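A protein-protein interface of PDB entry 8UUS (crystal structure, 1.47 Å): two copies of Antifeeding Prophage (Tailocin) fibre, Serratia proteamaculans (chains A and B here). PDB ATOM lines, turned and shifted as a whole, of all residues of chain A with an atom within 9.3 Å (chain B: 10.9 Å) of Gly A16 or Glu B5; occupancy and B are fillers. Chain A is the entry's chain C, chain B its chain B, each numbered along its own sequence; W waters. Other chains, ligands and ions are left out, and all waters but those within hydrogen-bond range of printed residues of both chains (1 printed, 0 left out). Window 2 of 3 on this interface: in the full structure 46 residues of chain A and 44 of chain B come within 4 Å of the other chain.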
ATOM      1  N   ALA A   6     -23.465  -4.921  15.681  1.00  0.00           N
ATOM      2  CA  ALA A   6     -22.163  -5.493  15.365  1.00  0.00           C
ATOM      3  C   ALA A   6     -21.412  -4.548  14.439  1.00  0.00           C
ATOM      4  O   ALA A   6     -21.951  -4.127  13.411  1.00  0.00           O
ATOM      5  CB  ALA A   6     -22.323  -6.853  14.690  1.00  0.00           C
ATOM      6  N   LEU A  10     -16.429  -7.436  12.653  1.00  0.00           N
ATOM      7  CA  LEU A  10     -17.518  -8.394  12.607  1.00  0.00           C
ATOM      8  C   LEU A  10     -18.335  -8.209  11.336  1.00  0.00           C
ATOM      9  O   LEU A  10     -18.307  -7.160  10.683  1.00  0.00           O
ATOM     10  CB  LEU A  10     -18.422  -8.208  13.828  1.00  0.00           C
ATOM     11  CG  LEU A  10     -17.735  -8.350  15.187  1.00  0.00           C
ATOM     12  CD1 LEU A  10     -18.770  -8.111  16.282  1.00  0.00           C
ATOM     13  CD2 LEU A  10     -17.072  -9.712  15.335  1.00  0.00           C
ATOM     14  N   GLN A  11     -19.051  -9.269  10.978  1.00  0.00           N
ATOM     15  CA  GLN A  11     -19.985  -9.207   9.868  1.00  0.00           C
ATOM     16  C   GLN A  11     -21.232  -9.993  10.227  1.00  0.00           C
ATOM     17  O   GLN A  11     -21.213 -10.875  11.095  1.00  0.00           O
ATOM     18  CB  GLN A  11     -19.361  -9.693   8.558  1.00  0.00           C
ATOM     19  CG  GLN A  11     -18.937 -11.122   8.557  1.00  0.00           C
ATOM     20  CD  GLN A  11     -18.254 -11.494   7.264  1.00  0.00           C
ATOM     21  OE1 GLN A  11     -18.347 -10.767   6.271  1.00  0.00           O
ATOM     22  NE2 GLN A  11     -17.555 -12.625   7.266  1.00  0.00           N
ATOM     23  N   VAL A  12     -22.324  -9.655   9.552  1.00  0.00           N
ATOM     24  CA  VAL A  12     -23.637 -10.188   9.880  1.00  0.00           C
ATOM     25  C   VAL A  12     -24.219 -10.821   8.630  1.00  0.00           C
ATOM     26  O   VAL A  12     -24.185 -10.223   7.549  1.00  0.00           O
ATOM     27  CB  VAL A  12     -24.567  -9.091  10.420  1.00  0.00           C
ATOM     28  CG1 VAL A  12     -25.885  -9.693  10.882  1.00  0.00           C
ATOM     29  CG2 VAL A  12     -23.894  -8.320  11.565  1.00  0.00           C
ATOM     30  N   THR A  13     -24.718 -12.041   8.774  1.00  0.00           N
ATOM     31  CA  THR A  13     -25.505 -12.706   7.745  1.00  0.00           C
ATOM     32  C   THR A  13     -26.808 -13.173   8.374  1.00  0.00           C
ATOM     33  O   THR A  13     -27.048 -12.996   9.576  1.00  0.00           O
ATOM     34  CB  THR A  13     -24.773 -13.924   7.161  1.00  0.00           C
ATOM     35  OG1 THR A  13     -24.766 -14.980   8.130  1.00  0.00           O
ATOM     36  CG2 THR A  13     -23.343 -13.571   6.765  1.00  0.00           C
ATOM     37  N   ALA A  14     -27.650 -13.810   7.548  1.00  0.00           N
ATOM     38  CA  ALA A  14     -28.883 -14.388   8.070  1.00  0.00           C
ATOM     39  C   ALA A  14     -28.613 -15.445   9.128  1.00  0.00           C
ATOM     40  O   ALA A  14     -29.511 -15.766   9.910  1.00  0.00           O
ATOM     41  CB  ALA A  14     -29.723 -14.971   6.930  1.00  0.00           C
ATOM     42  N   SER A  15     -27.397 -15.985   9.174  1.00  0.00           N
ATOM     43  CA  SER A  15     -27.023 -16.991  10.159  1.00  0.00           C
ATOM     44  C   SER A  15     -26.452 -16.404  11.448  1.00  0.00           C
ATOM     45  O   SER A  15     -26.227 -17.156  12.400  1.00  0.00           O
ATOM     46  CB  SER A  15     -26.006 -17.956   9.545  1.00  0.00           C
ATOM     47  OG  SER A  15     -26.595 -18.694   8.489  1.00  0.00           O
ATOM     48  N   GLY A  16     -26.200 -15.096  11.510  1.00  0.00           N
ATOM     49  CA  GLY A  16     -25.748 -14.503  12.747  1.00  0.00           C
ATOM     50  C   GLY A  16     -24.505 -13.670  12.531  1.00  0.00           C
ATOM     51  O   GLY A  16     -24.182 -13.284  11.402  1.00  0.00           O
ATOM     52  N   VAL A  17     -23.813 -13.389  13.634  1.00  0.00           N
ATOM     53  CA  VAL A  17     -22.646 -12.510  13.642  1.00  0.00           C
ATOM     54  C   VAL A  17     -21.389 -13.362  13.637  1.00  0.00           C
ATOM     55  O   VAL A  17     -21.282 -14.334  14.393  1.00  0.00           O
ATOM     56  CB  VAL A  17     -22.670 -11.582  14.862  1.00  0.00           C
ATOM     57  CG1 VAL A  17     -21.476 -10.631  14.826  1.00  0.00           C
ATOM     58  CG2 VAL A  17     -23.970 -10.812  14.880  1.00  0.00           C
ATOM     59  N   SER A  18     -20.430 -12.993  12.794  1.00  0.00           N
ATOM     60  CA  SER A  18     -19.176 -13.714  12.692  1.00  0.00           C
ATOM     61  C   SER A  18     -18.041 -12.703  12.648  1.00  0.00           C
ATOM     62  O   SER A  18     -18.260 -11.493  12.521  1.00  0.00           O
ATOM     63  CB  SER A  18     -19.161 -14.625  11.451  1.00  0.00           C
ATOM     64  OG  SER A  18     -19.371 -13.863  10.272  1.00  0.00           O
ATOM     65  N   VAL A  19     -16.822 -13.207  12.778  1.00  0.00           N
ATOM     66  CA  VAL A  19     -15.633 -12.390  12.540  1.00  0.00           C
ATOM     67  C   VAL A  19     -15.386 -12.341  11.043  1.00  0.00           C
ATOM     68  O   VAL A  19     -15.401 -13.380  10.365  1.00  0.00           O
ATOM     69  CB  VAL A  19     -14.413 -12.976  13.270  1.00  0.00           C
ATOM     70  CG1 VAL A  19     -13.158 -12.165  12.954  1.00  0.00           C
ATOM     71  CG2 VAL A  19     -14.650 -13.023  14.772  1.00  0.00           C
ATOM     72  N   GLU B   5     -27.569 -14.564  16.659  1.00  0.00           N
ATOM     73  CA  GLU B   5     -26.608 -15.356  17.419  1.00  0.00           C
ATOM     74  C   GLU B   5     -25.193 -15.221  16.865  1.00  0.00           C
ATOM     75  O   GLU B   5     -24.953 -14.459  15.926  1.00  0.00           O
ATOM     76  CB  GLU B   5     -27.025 -16.828  17.429  1.00  0.00           C
ATOM     77  N   ALA B   6     -24.262 -15.964  17.458  1.00  0.00           N
ATOM     78  CA  ALA B   6     -22.873 -15.981  17.024  1.00  0.00           C
ATOM     79  C   ALA B   6     -22.627 -17.130  16.052  1.00  0.00           C
ATOM     80  O   ALA B   6     -23.224 -18.205  16.170  1.00  0.00           O
ATOM     81  CB  ALA B   6     -21.951 -16.157  18.228  1.00  0.00           C
ATOM     82  N   SER B   7     -21.745 -16.889  15.076  1.00  0.00           N
ATOM     83  CA  SER B   7     -21.183 -17.978  14.275  1.00  0.00           C
ATOM     84  C   SER B   7     -19.665 -17.862  14.113  1.00  0.00           C
ATOM     85  O   SER B   7     -18.954 -17.656  15.101  1.00  0.00           O
ATOM     86  CB  SER B   7     -21.922 -18.192  12.945  1.00  0.00           C
ATOM     87  OG  SER B   7     -22.216 -16.983  12.273  1.00  0.00           O
ATOM     88  N   LYS B   8     -19.161 -17.989  12.885  1.00  0.00           N
ATOM     89  CA  LYS B   8     -17.746 -18.296  12.655  1.00  0.00           C
ATOM     90  C   LYS B   8     -16.801 -17.270  13.283  1.00  0.00           C
ATOM     91  O   LYS B   8     -16.914 -16.069  13.026  1.00  0.00           O
ATOM     92  CB  LYS B   8     -17.484 -18.342  11.153  1.00  0.00           C
ATOM     93  CG  LYS B   8     -18.440 -19.218  10.368  1.00  0.00           C
ATOM     94  CD  LYS B   8     -17.944 -19.395   8.944  1.00  0.00           C
ATOM     95  CE  LYS B   8     -18.085 -18.104   8.149  1.00  0.00           C
ATOM     96  NZ  LYS B   8     -18.378 -18.336   6.703  1.00  0.00           N
ATOM     97  N   GLY B   9     -15.821 -17.763  14.051  1.00  0.00           N
ATOM     98  CA  GLY B   9     -14.841 -16.928  14.720  1.00  0.00           C
ATOM     99  C   GLY B   9     -15.246 -16.473  16.103  1.00  0.00           C
ATOM    100  O   GLY B   9     -14.390 -16.005  16.860  1.00  0.00           O
ATOM    101  N   LEU B  10     -16.522 -16.592  16.443  1.00  0.00           N
ATOM    102  CA  LEU B  10     -17.041 -16.237  17.750  1.00  0.00           C
ATOM    103  C   LEU B  10     -17.503 -17.501  18.459  1.00  0.00           C
ATOM    104  O   LEU B  10     -17.743 -18.536  17.837  1.00  0.00           O
ATOM    105  CB  LEU B  10     -18.204 -15.239  17.629  1.00  0.00           C
ATOM    106  CG  LEU B  10     -17.909 -13.886  16.961  1.00  0.00           C
ATOM    107  CD1 LEU B  10     -19.135 -12.999  16.965  1.00  0.00           C
ATOM    108  CD2 LEU B  10     -16.751 -13.180  17.645  1.00  0.00           C
ATOM    109  N   GLN B  11     -17.602 -17.410  19.779  1.00  0.00           N
ATOM    110  CA  GLN B  11     -18.079 -18.517  20.590  1.00  0.00           C
ATOM    111  C   GLN B  11     -18.847 -17.938  21.766  1.00  0.00           C
ATOM    112  O   GLN B  11     -18.648 -16.783  22.154  1.00  0.00           O
ATOM    113  CB  GLN B  11     -16.901 -19.367  21.076  1.00  0.00           C
ATOM    114  CG  GLN B  11     -15.936 -18.548  21.906  1.00  0.00           C
ATOM    115  CD  GLN B  11     -14.742 -19.324  22.411  1.00  0.00           C
ATOM    116  OE1 GLN B  11     -14.604 -20.524  22.153  1.00  0.00           O
ATOM    117  NE2 GLN B  11     -13.851 -18.628  23.129  1.00  0.00           N
ATOM    118  N   VAL B  12     -19.735 -18.752  22.326  1.00  0.00           N
ATOM    119  CA  VAL B  12     -20.538 -18.373  23.481  1.00  0.00           C
ATOM    120  C   VAL B  12     -20.244 -19.360  24.598  1.00  0.00           C
ATOM    121  O   VAL B  12     -20.329 -20.579  24.397  1.00  0.00           O
ATOM    122  CB  VAL B  12     -22.041 -18.351  23.148  1.00  0.00           C
ATOM    123  CG1 VAL B  12     -22.851 -17.992  24.386  1.00  0.00           C
ATOM    124  CG2 VAL B  12     -22.329 -17.370  22.032  1.00  0.00           C
ATOM    125  N   GLY B  16     -20.220 -15.188  28.195  1.00  0.00           N
ATOM    126  CA  GLY B  16     -20.779 -14.375  27.131  1.00  0.00           C
ATOM    127  C   GLY B  16     -20.174 -14.698  25.779  1.00  0.00           C
ATOM    128  O   GLY B  16     -19.660 -15.791  25.537  1.00  0.00           O
ATOM    129  N   VAL B  17     -20.243 -13.725  24.876  1.00  0.00           N
ATOM    130  CA  VAL B  17     -19.707 -13.922  23.529  1.00  0.00           C
ATOM    131  C   VAL B  17     -18.248 -13.474  23.495  1.00  0.00           C
ATOM    132  O   VAL B  17     -17.906 -12.392  23.989  1.00  0.00           O
ATOM    133  CB  VAL B  17     -20.563 -13.208  22.465  1.00  0.00           C
ATOM    134  CG1 VAL B  17     -20.722 -11.711  22.754  1.00  0.00           C
ATOM    135  CG2 VAL B  17     -20.005 -13.458  21.069  1.00  0.00           C
ATOM    136  N   SER B  18     -17.377 -14.320  22.939  1.00  0.00           N
ATOM    137  CA  SER B  18     -15.959 -13.997  22.822  1.00  0.00           C
ATOM    138  C   SER B  18     -15.456 -14.394  21.438  1.00  0.00           C
ATOM    139  O   SER B  18     -16.121 -15.122  20.691  1.00  0.00           O
ATOM    140  CB  SER B  18     -15.118 -14.696  23.894  1.00  0.00           C
ATOM    141  OG  SER B  18     -15.227 -16.108  23.779  1.00  0.00           O
HETATM  142  O   HOH W   1     -22.267 -16.759   9.273  1.00  0.00           O
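O of Glu B5 is in hydrogen-bond range of N of Val A17 (2.8 Å). The backbone NH of Ser B7 sits at hydrogen-bond distance from the backbone carbonyl oxygen of Val A17 (2.7 Å). O of Lys B8 is in hydrogen-bond range of N of Val A19 (2.9 Å).
The backbone carbonyl oxygen (O) of Ser A18 sits at hydrogen-bond distance from the backbone NH (N) of Gln A11, 2.8 Å away.
CA of Gly A16 touches O of Glu B5 (3.3 Å). Ala B6 touches Val A17. Leu B10 touches Val A17. Ser A18 touches Ser B7. CB of Ser A18 touches O of Lys B8, at 3.1 Å. Val A19 touches Gly B9 (CG2 to O, 3.6 Å). CD2 of Leu B10 touches CG2 of Val A19 (3.6 Å).
Gly A16 touches just one residue of chain B: Glu B5 (3.3 Å). Glu B5 touches two residues of chain A. Thr A13 touches none of the printed residues of chain B. No residue of chain B comes within 4 Å of Ala A14. Of the printed residues of chain B, Val A17 touches Glu B5 (2.8 Å), Ala B6 (3.5 Å), Ser B7 (2.7 Å) and Leu B10 (3.6 Å). Ser A18 touches just these residues of chain B: Ser B7 and Lys B8. Ala B6 touches just one residue of chain A: Val A17. Printed residues of chain A within 4 Å of Ser B7: Val A17 (2.7 Å) and Ser A18 (3.9 Å). Of the printed residues of chain A, Gly B9 touches Val A19 (3.6 Å). Of the printed residues of chain A, Lys B8 touches Ser A18 (3.1 Å) and Val A19 (2.9 Å). Printed residues of chain B within 4 Å of Val A19: Lys B8 (2.9 Å), Gly B9 (3.6 Å) and Leu B10 (3.6 Å). Gly B16 touches none of the printed residues of chain A. The nearest printed residue of chain A that does not touch Leu B10 is Leu A10 (4.2 Å).
Printed residues of chain B that touch a printed residue of chain A: Glu B5, Ala B6, Ser B7, Lys B8, Gly B9 and Leu B10. Of the 11 printed residues of chain A, 4 touch a printed residue of chain B.
Val A17 touches Ala B6, but with the chains exchanged Ala A6 does not touch Val B17 (9.5 Å). Val A17 touches Leu B10, but with the chains exchanged Leu A10 does not touch Val B17 (7.3 Å). 7 positions are printed for both chains. Of the 10 pairs that touch across the chains among the printed residues, none has its exchanged pair printed and touching as well.
Water W1 bridges the side-chain hydroxyl of Ser B7 and the side-chain hydroxyl of Thr A13.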
